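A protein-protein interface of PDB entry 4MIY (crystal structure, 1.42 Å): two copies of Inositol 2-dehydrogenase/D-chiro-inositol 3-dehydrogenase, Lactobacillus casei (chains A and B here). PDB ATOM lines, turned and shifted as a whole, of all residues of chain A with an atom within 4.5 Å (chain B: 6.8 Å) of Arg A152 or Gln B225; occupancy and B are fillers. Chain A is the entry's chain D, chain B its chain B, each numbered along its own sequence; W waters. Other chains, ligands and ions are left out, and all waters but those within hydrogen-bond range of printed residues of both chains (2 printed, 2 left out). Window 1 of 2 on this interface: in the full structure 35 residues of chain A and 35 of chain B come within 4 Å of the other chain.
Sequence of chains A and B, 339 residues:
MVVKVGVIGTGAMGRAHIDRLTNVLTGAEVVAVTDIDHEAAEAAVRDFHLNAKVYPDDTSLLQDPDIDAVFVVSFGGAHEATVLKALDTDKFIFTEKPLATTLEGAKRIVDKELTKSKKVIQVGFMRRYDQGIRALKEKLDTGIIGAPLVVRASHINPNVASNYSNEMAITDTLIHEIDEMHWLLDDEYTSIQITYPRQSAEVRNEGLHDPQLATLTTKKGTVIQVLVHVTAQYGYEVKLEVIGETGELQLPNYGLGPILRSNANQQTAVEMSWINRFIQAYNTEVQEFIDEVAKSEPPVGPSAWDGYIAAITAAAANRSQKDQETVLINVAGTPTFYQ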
ATOM      1  N   VAL A 150      12.474  -7.143  11.170  1.00  0.00           N
ATOM      2  CA  VAL A 150      11.347  -7.271  12.081  1.00  0.00           C
ATOM      3  C   VAL A 150      10.958  -5.877  12.587  1.00  0.00           C
ATOM      4  O   VAL A 150      11.797  -5.043  12.762  1.00  0.00           O
ATOM      5  CB  VAL A 150      11.677  -8.158  13.295  1.00  0.00           C
ATOM      6  CG1 VAL A 150      10.520  -8.231  14.249  1.00  0.00           C
ATOM      7  CG2 VAL A 150      12.049  -9.565  12.870  1.00  0.00           C
ATOM      8  N   VAL A 151       9.662  -5.676  12.776  1.00  0.00           N
ATOM      9  CA  VAL A 151       9.134  -4.485  13.402  1.00  0.00           C
ATOM     10  C   VAL A 151       8.327  -4.911  14.621  1.00  0.00           C
ATOM     11  O   VAL A 151       7.569  -5.799  14.552  1.00  0.00           O
ATOM     12  CB  VAL A 151       8.234  -3.663  12.472  1.00  0.00           C
ATOM     13  CG1 VAL A 151       7.724  -2.404  13.189  1.00  0.00           C
ATOM     14  CG2 VAL A 151       8.957  -3.254  11.249  1.00  0.00           C
ATOM     15  N   ARG A 152       8.590  -4.270  15.739  1.00  0.00           N
ATOM     16  CA  ARG A 152       7.810  -4.480  16.923  1.00  0.00           C
ATOM     17  C   ARG A 152       7.119  -3.185  17.288  1.00  0.00           C
ATOM     18  O   ARG A 152       7.738  -2.185  17.385  1.00  0.00           O
ATOM     19  CB  ARG A 152       8.650  -5.026  18.072  1.00  0.00           C
ATOM     20  CG  ARG A 152       9.199  -6.353  17.752  1.00  0.00           C
ATOM     21  CD  ARG A 152       9.950  -6.969  18.835  1.00  0.00           C
ATOM     22  NE  ARG A 152       9.497  -8.323  19.053  1.00  0.00           N
ATOM     23  CZ  ARG A 152       9.905  -9.066  20.056  1.00  0.00           C
ATOM     24  NH1 ARG A 152      10.796  -8.607  20.884  1.00  0.00           N
ATOM     25  NH2 ARG A 152       9.454 -10.283  20.195  1.00  0.00           N
ATOM     26  N   ALA A 153       5.814  -3.262  17.466  1.00  0.00           N
ATOM     27  CA  ALA A 153       5.000  -2.104  17.770  1.00  0.00           C
ATOM     28  C   ALA A 153       4.022  -2.380  18.906  1.00  0.00           C
ATOM     29  O   ALA A 153       3.586  -3.482  19.081  1.00  0.00           O
ATOM     30  CB  ALA A 153       4.241  -1.671  16.552  1.00  0.00           C
ATOM     31  N   LEU A 213      -2.754  -9.775  19.765  1.00  0.00           N
ATOM     32  CA  LEU A 213      -1.497  -9.800  19.044  1.00  0.00           C
ATOM     33  C   LEU A 213      -1.729  -9.941  17.543  1.00  0.00           C
ATOM     34  O   LEU A 213      -2.471 -10.769  17.113  1.00  0.00           O
ATOM     35  CB  LEU A 213      -0.595 -10.912  19.546  1.00  0.00           C
ATOM     36  CG  LEU A 213      -0.228 -10.865  21.021  1.00  0.00           C
ATOM     37  CD1 LEU A 213       0.476 -12.147  21.444  1.00  0.00           C
ATOM     38  CD2 LEU A 213       0.613  -9.681  21.318  1.00  0.00           C
ATOM     39  N   GLN A 225       5.153  -7.483  14.428  1.00  0.00           N
ATOM     40  CA  GLN A 225       4.446  -7.936  15.614  1.00  0.00           C
ATOM     41  C   GLN A 225       3.887  -6.735  16.381  1.00  0.00           C
ATOM     42  O   GLN A 225       4.617  -6.014  16.966  1.00  0.00           O
ATOM     43  CB  GLN A 225       5.399  -8.671  16.545  1.00  0.00           C
ATOM     44  CG  GLN A 225       5.989  -9.951  15.981  1.00  0.00           C
ATOM     45  CD  GLN A 225       6.848 -10.705  16.976  1.00  0.00           C
ATOM     46  OE1 GLN A 225       7.609 -10.151  17.704  1.00  0.00           O
ATOM     47  NE2 GLN A 225       6.674 -11.986  17.001  1.00  0.00           N
ATOM     48  N   LYS A 239       4.421   2.701  20.601  1.00  0.00           N
ATOM     49  CA  LYS A 239       5.815   2.286  20.598  1.00  0.00           C
ATOM     50  C   LYS A 239       6.144   1.672  19.228  1.00  0.00           C
ATOM     51  O   LYS A 239       5.328   1.062  18.616  1.00  0.00           O
ATOM     52  CB  LYS A 239       6.093   1.270  21.690  1.00  0.00           C
ATOM     53  CG  LYS A 239       5.746   1.683  23.104  1.00  0.00           C
ATOM     54  CD  LYS A 239       6.156   0.593  24.044  1.00  0.00           C
ATOM     55  CE  LYS A 239       5.627   0.757  25.428  1.00  0.00           C
ATOM     56  NZ  LYS A 239       6.169  -0.275  26.281  1.00  0.00           N
ATOM     57  N   LEU A 240       7.367   1.894  18.795  1.00  0.00           N
ATOM     58  CA  LEU A 240       7.858   1.453  17.510  1.00  0.00           C
ATOM     59  C   LEU A 240       9.349   1.174  17.563  1.00  0.00           C
ATOM     60  O   LEU A 240      10.098   2.011  17.894  1.00  0.00           O
ATOM     61  CB  LEU A 240       7.557   2.487  16.437  1.00  0.00           C
ATOM     62  CG  LEU A 240       7.999   2.217  15.018  1.00  0.00           C
ATOM     63  CD1 LEU A 240       7.289   1.026  14.480  1.00  0.00           C
ATOM     64  CD2 LEU A 240       7.710   3.400  14.238  1.00  0.00           C
ATOM     65  N   GLU A 241       9.698  -0.038  17.171  1.00  0.00           N
ATOM     66  CA  GLU A 241      11.065  -0.502  17.102  1.00  0.00           C
ATOM     67  C   GLU A 241      11.270  -1.232  15.771  1.00  0.00           C
ATOM     68  O   GLU A 241      10.524  -2.083  15.425  1.00  0.00           O
ATOM     69  CB  GLU A 241      11.343  -1.416  18.281  1.00  0.00           C
ATOM     70  CG  GLU A 241      12.655  -2.131  18.283  1.00  0.00           C
ATOM     71  CD  GLU A 241      12.780  -3.147  19.409  1.00  0.00           C
ATOM     72  OE1 GLU A 241      11.770  -3.625  19.880  1.00  0.00           O
ATOM     73  OE2 GLU A 241      13.888  -3.467  19.813  1.00  0.00           O
ATOM     74  N   VAL B 150       1.285 -10.823  28.340  1.00  0.00           N
ATOM     75  CA  VAL B 150       2.203 -10.975  27.243  1.00  0.00           C
ATOM     76  C   VAL B 150       3.606 -10.647  27.769  1.00  0.00           C
ATOM     77  O   VAL B 150       3.782  -9.790  28.595  1.00  0.00           O
ATOM     78  CB  VAL B 150       1.846 -10.022  26.087  1.00  0.00           C
ATOM     79  CG1 VAL B 150       2.850 -10.088  24.978  1.00  0.00           C
ATOM     80  CG2 VAL B 150       0.504 -10.319  25.518  1.00  0.00           C
ATOM     81  N   VAL B 151       4.595 -11.378  27.274  1.00  0.00           N
ATOM     82  CA  VAL B 151       5.986 -11.077  27.523  1.00  0.00           C
ATOM     83  C   VAL B 151       6.649 -10.859  26.164  1.00  0.00           C
ATOM     84  O   VAL B 151       6.469 -11.629  25.284  1.00  0.00           O
ATOM     85  CB  VAL B 151       6.699 -12.224  28.267  1.00  0.00           C
ATOM     86  CG1 VAL B 151       8.113 -11.897  28.446  1.00  0.00           C
ATOM     87  CG2 VAL B 151       6.070 -12.442  29.593  1.00  0.00           C
ATOM     88  N   ARG B 152       7.365  -9.756  26.032  1.00  0.00           N
ATOM     89  CA  ARG B 152       8.144  -9.474  24.839  1.00  0.00           C
ATOM     90  C   ARG B 152       9.587  -9.386  25.227  1.00  0.00           C
ATOM     91  O   ARG B 152       9.938  -8.640  26.086  1.00  0.00           O
ATOM     92  CB  ARG B 152       7.699  -8.204  24.180  1.00  0.00           C
ATOM     93  CG  ARG B 152       6.275  -8.253  23.760  1.00  0.00           C
ATOM     94  CD  ARG B 152       5.917  -7.054  22.956  1.00  0.00           C
ATOM     95  NE  ARG B 152       5.300  -7.461  21.736  1.00  0.00           N
ATOM     96  CZ  ARG B 152       4.920  -6.667  20.762  1.00  0.00           C
ATOM     97  NH1 ARG B 152       5.060  -5.396  20.846  1.00  0.00           N
ATOM     98  NH2 ARG B 152       4.353  -7.190  19.724  1.00  0.00           N
ATOM     99  N   ALA B 153      10.413 -10.185  24.580  1.00  0.00           N
ATOM    100  CA  ALA B 153      11.816 -10.302  24.935  1.00  0.00           C
ATOM    101  C   ALA B 153      12.704 -10.312  23.699  1.00  0.00           C
ATOM    102  O   ALA B 153      12.249 -10.630  22.637  1.00  0.00           O
ATOM    103  CB  ALA B 153      12.033 -11.519  25.749  1.00  0.00           C
ATOM    104  N   SER B 154      13.949  -9.904  23.884  1.00  0.00           N
ATOM    105  CA  SER B 154      14.972  -9.961  22.842  1.00  0.00           C
ATOM    106  C   SER B 154      16.256 -10.570  23.367  1.00  0.00           C
ATOM    107  O   SER B 154      16.670 -10.289  24.433  1.00  0.00           O
ATOM    108  CB  SER B 154      15.291  -8.598  22.225  1.00  0.00           C
ATOM    109  OG  SER B 154      14.166  -8.020  21.620  1.00  0.00           O
ATOM    110  N   MET B 181      11.522 -17.962  31.374  1.00  0.00           N
ATOM    111  CA  MET B 181      10.152 -17.485  31.322  1.00  0.00           C
ATOM    112  C   MET B 181       9.203 -18.269  32.210  1.00  0.00           C
ATOM    113  O   MET B 181       8.361 -17.703  32.827  1.00  0.00           O
ATOM    114  CB  MET B 181       9.633 -17.421  29.909  1.00  0.00           C
ATOM    115  CG  MET B 181      10.418 -16.581  28.999  1.00  0.00           C
ATOM    116  SD  MET B 181      10.486 -14.864  29.509  1.00  0.00           S
ATOM    117  CE  MET B 181      11.611 -14.220  28.289  1.00  0.00           C
ATOM    118  N   LEU B 213      12.004 -15.788  15.291  1.00  0.00           N
ATOM    119  CA  LEU B 213      11.000 -15.400  16.241  1.00  0.00           C
ATOM    120  C   LEU B 213      10.446 -16.609  16.917  1.00  0.00           C
ATOM    121  O   LEU B 213       9.969 -17.484  16.291  1.00  0.00           O
ATOM    122  CB  LEU B 213       9.871 -14.626  15.562  1.00  0.00           C
ATOM    123  CG  LEU B 213      10.251 -13.314  14.914  1.00  0.00           C
ATOM    124  CD1 LEU B 213       9.154 -12.850  14.000  1.00  0.00           C
ATOM    125  CD2 LEU B 213      10.532 -12.313  15.939  1.00  0.00           C
ATOM    126  N   ALA B 214      10.518 -16.623  18.229  1.00  0.00           N
ATOM    127  CA  ALA B 214       9.973 -17.697  19.008  1.00  0.00           C
ATOM    128  C   ALA B 214       8.727 -17.239  19.769  1.00  0.00           C
ATOM    129  O   ALA B 214       8.753 -16.240  20.442  1.00  0.00           O
ATOM    130  CB  ALA B 214      11.008 -18.211  19.954  1.00  0.00           C
ATOM    131  N   THR B 215       7.664 -17.986  19.626  1.00  0.00           N
ATOM    132  CA  THR B 215       6.446 -17.723  20.359  1.00  0.00           C
ATOM    133  C   THR B 215       6.098 -18.894  21.239  1.00  0.00           C
ATOM    134  O   THR B 215       5.968 -19.995  20.782  1.00  0.00           O
ATOM    135  CB  THR B 215       5.300 -17.419  19.426  1.00  0.00           C
ATOM    136  OG1 THR B 215       5.631 -16.281  18.629  1.00  0.00           O
ATOM    137  CG2 THR B 215       4.043 -17.182  20.232  1.00  0.00           C
ATOM    138  N   LEU B 216       5.989 -18.636  22.525  1.00  0.00           N
ATOM    139  CA  LEU B 216       5.587 -19.641  23.474  1.00  0.00           C
ATOM    140  C   LEU B 216       4.273 -19.302  24.128  1.00  0.00           C
ATOM    141  O   LEU B 216       4.015 -18.180  24.435  1.00  0.00           O
ATOM    142  CB  LEU B 216       6.647 -19.861  24.562  1.00  0.00           C
ATOM    143  CG  LEU B 216       8.008 -20.400  24.163  1.00  0.00           C
ATOM    144  CD1 LEU B 216       8.843 -19.357  23.597  1.00  0.00           C
ATOM    145  CD2 LEU B 216       8.630 -20.956  25.368  1.00  0.00           C
ATOM    146  N   VAL B 223       1.272 -15.220  26.466  1.00  0.00           N
ATOM    147  CA  VAL B 223       2.028 -15.420  25.259  1.00  0.00           C
ATOM    148  C   VAL B 223       3.383 -14.719  25.373  1.00  0.00           C
ATOM    149  O   VAL B 223       3.474 -13.576  25.706  1.00  0.00           O
ATOM    150  CB  VAL B 223       1.264 -14.923  24.052  1.00  0.00           C
ATOM    151  CG1 VAL B 223       2.121 -15.038  22.807  1.00  0.00           C
ATOM    152  CG2 VAL B 223      -0.006 -15.705  23.868  1.00  0.00           C
ATOM    153  N   ILE B 224       4.428 -15.477  25.089  1.00  0.00           N
ATOM    154  CA  ILE B 224       5.774 -14.980  25.062  1.00  0.00           C
ATOM    155  C   ILE B 224       6.290 -14.862  23.639  1.00  0.00           C
ATOM    156  O   ILE B 224       6.299 -15.801  22.928  1.00  0.00           O
ATOM    157  CB  ILE B 224       6.718 -15.914  25.851  1.00  0.00           C
ATOM    158  CG1 ILE B 224       6.195 -16.101  27.271  1.00  0.00           C
ATOM    159  CG2 ILE B 224       8.102 -15.398  25.858  1.00  0.00           C
ATOM    160  CD1 ILE B 224       6.375 -17.464  27.806  1.00  0.00           C
ATOM    161  N   GLN B 225       6.738 -13.673  23.286  1.00  0.00           N
ATOM    162  CA  GLN B 225       7.341 -13.397  21.999  1.00  0.00           C
ATOM    163  C   GLN B 225       8.809 -13.019  22.162  1.00  0.00           C
ATOM    164  O   GLN B 225       9.118 -11.996  22.656  1.00  0.00           O
ATOM    165  CB  GLN B 225       6.589 -12.275  21.299  1.00  0.00           C
ATOM    166  CG  GLN B 225       5.154 -12.501  21.036  1.00  0.00           C
ATOM    167  CD  GLN B 225       4.513 -11.336  20.322  1.00  0.00           C
ATOM    168  OE1 GLN B 225       4.763 -10.219  20.655  1.00  0.00           O
ATOM    169  NE2 GLN B 225       3.739 -11.607  19.315  1.00  0.00           N
ATOM    170  N   VAL B 226       9.696 -13.898  21.711  1.00  0.00           N
ATOM    171  CA  VAL B 226      11.126 -13.658  21.767  1.00  0.00           C
ATOM    172  C   VAL B 226      11.710 -13.438  20.403  1.00  0.00           C
ATOM    173  O   VAL B 226      11.464 -14.195  19.522  1.00  0.00           O
ATOM    174  CB  VAL B 226      11.911 -14.816  22.407  1.00  0.00           C
ATOM    175  CG1 VAL B 226      13.314 -14.410  22.619  1.00  0.00           C
ATOM    176  CG2 VAL B 226      11.256 -15.258  23.717  1.00  0.00           C
ATOM    177  N   LEU B 227      12.472 -12.371  20.273  1.00  0.00           N
ATOM    178  CA  LEU B 227      13.285 -12.109  19.101  1.00  0.00           C
ATOM    179  C   LEU B 227      14.695 -12.622  19.367  1.00  0.00           C
ATOM    180  O   LEU B 227      15.325 -12.212  20.291  1.00  0.00           O
ATOM    181  CB  LEU B 227      13.358 -10.622  18.801  1.00  0.00           C
ATOM    182  CG  LEU B 227      14.382 -10.179  17.760  1.00  0.00           C
ATOM    183  CD1 LEU B 227      14.024 -10.661  16.411  1.00  0.00           C
ATOM    184  CD2 LEU B 227      14.511  -8.690  17.767  1.00  0.00           C
ATOM    185  N   VAL B 228      15.135 -13.565  18.550  1.00  0.00           N
ATOM    186  CA  VAL B 228      16.499 -14.055  18.566  1.00  0.00           C
ATOM    187  C   VAL B 228      17.224 -13.504  17.346  1.00  0.00           C
ATOM    188  O   VAL B 228      16.840 -13.750  16.248  1.00  0.00           O
ATOM    189  CB  VAL B 228      16.527 -15.567  18.556  1.00  0.00           C
ATOM    190  CG1 VAL B 228      17.956 -16.084  18.511  1.00  0.00           C
ATOM    191  CG2 VAL B 228      15.790 -16.100  19.753  1.00  0.00           C
ATOM    192  N   LYS B 239      16.739  -8.013  26.423  1.00  0.00           N
ATOM    193  CA  LYS B 239      15.600  -7.134  26.671  1.00  0.00           C
ATOM    194  C   LYS B 239      14.430  -7.967  27.155  1.00  0.00           C
ATOM    195  O   LYS B 239      14.243  -9.049  26.732  1.00  0.00           O
ATOM    196  CB  LYS B 239      15.187  -6.372  25.414  1.00  0.00           C
ATOM    197  CG  LYS B 239      16.257  -5.557  24.734  1.00  0.00           C
ATOM    198  CD  LYS B 239      15.681  -4.804  23.581  1.00  0.00           C
ATOM    199  CE  LYS B 239      16.741  -4.230  22.709  1.00  0.00           C
ATOM    200  NZ  LYS B 239      16.213  -3.424  21.649  1.00  0.00           N
HETATM  201  O   HOH W   1       8.267 -13.858  18.656  1.00  0.00           O
HETATM  202  O   HOH W   2      15.254  -5.922  20.097  1.00  0.00           O
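NH1 of Arg B152 is in hydrogen-bond range of O of Ala A153 (3.0 Å). O of Gln A225 sits at hydrogen-bond distance from NH2 of Arg B152, at 3.0 Å. The guanidinium group of Arg A152 is in hydrogen-bond range of the backbone carbonyl oxygen of Ala B153. The guanidinium group (NH1) of Arg A152 lies within hydrogen-bond range of the side-chain hydroxyl (OG) of Ser B154 (3.5 Å). The backbone carbonyl oxygen of Gln B225 lies within hydrogen-bond range of the guanidinium group of Arg A152 (3.0 Å). The side-chain amino group (NZ) of Lys B239 is in salt-bridge range of the side-chain carboxylate (OE2) of Glu A241 (3.0 Å).
The backbone carbonyl oxygen of Val B223 is in hydrogen-bond range of the backbone NH of Val B151 (2.9 Å). The guanidinium group of Arg B152 is in hydrogen-bond range of the side-chain amide oxygen of Gln B225 (3.0 Å). N of Ala B153 lies within hydrogen-bond range of O of Gln B225, 2.9 Å away. The backbone NH (N) of Ser B154 lies within hydrogen-bond range of the backbone carbonyl oxygen (O) of Lys B239, at 3.0 Å. The backbone carbonyl oxygen of Val A151 is in hydrogen-bond range of the backbone NH of Gln A225 (2.9 Å). The backbone NH (N) of Ala A153 lies within hydrogen-bond range of the backbone carbonyl oxygen (O) of Gln A225 (3.0 Å).
Arg A152 touches Val B226. Leu B227 touches Arg A152 (N to NH2, 3.7 Å). Val B223 touches Leu A213. Leu A213 touches Gln B225 (CD1 to NE2, 3.9 Å). NE2 of Gln A225 touches CD1 of Leu B213, 3.99 Å away. Gln A225 touches Gln B225.
Of chain B, only Ala B153 (3.0 Å), Ser B154 (3.5 Å), Gln B225 (3.0 Å), Val B226 (3.9 Å) and Leu B227 (3.7 Å) come within 4 Å of Arg A152. Printed residues of chain B within 4 Å of Gln A225: Arg B152 (3.0 Å), Leu B213 (3.99 Å) and Gln B225 (3.8 Å). Printed residues of chain A within 4 Å of Leu B213: Gln A225 (3.99 Å). Printed residues of chain A within 4 Å of Val B223: Leu A213. The nearest printed residue of chain A that does not touch Gln B225 is Ala A153 (7.0 Å).
Along chain A the printed residues that touch a printed residue of chain B span positions 152 to 241. Among the printed residues, Asp or Glu carboxylates within 4 Å of a Lys or Arg side-chain nitrogen of the other chain: Glu A241 with Lys B239 (3.0 Å).
Arg A152 touches Ala B153, and with the chains exchanged Ala A153 touches Arg B152. Arg A152 touches Gln B225, and with the chains exchanged Gln A225 touches Arg B152. Leu A213 touches Gln B225, and with the chains exchanged Gln A225 touches Leu B213. Gln A225 touches its own counterpart, Gln B225. Positions printed for both chains: 150, 151, 152, 153, 213, 225 and 239. Of the 12 pairs that touch across the chains among the printed residues, 7 have their exchanged pair printed and touching as well.
Water W2 lies within hydrogen-bond range of the side-chain hydroxyl (OG) of Ser B154 (2.8 Å), the side-chain carboxylate (OE2) of Glu A241 (2.8 Å) and the side-chain amino group (NZ) of Lys B239 (3.1 Å). Water W1 lies within hydrogen-bond range of the side-chain amide nitrogen of Gln A225, the backbone carbonyl oxygen of Ala B214 and the backbone carbonyl oxygen of Val B226.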
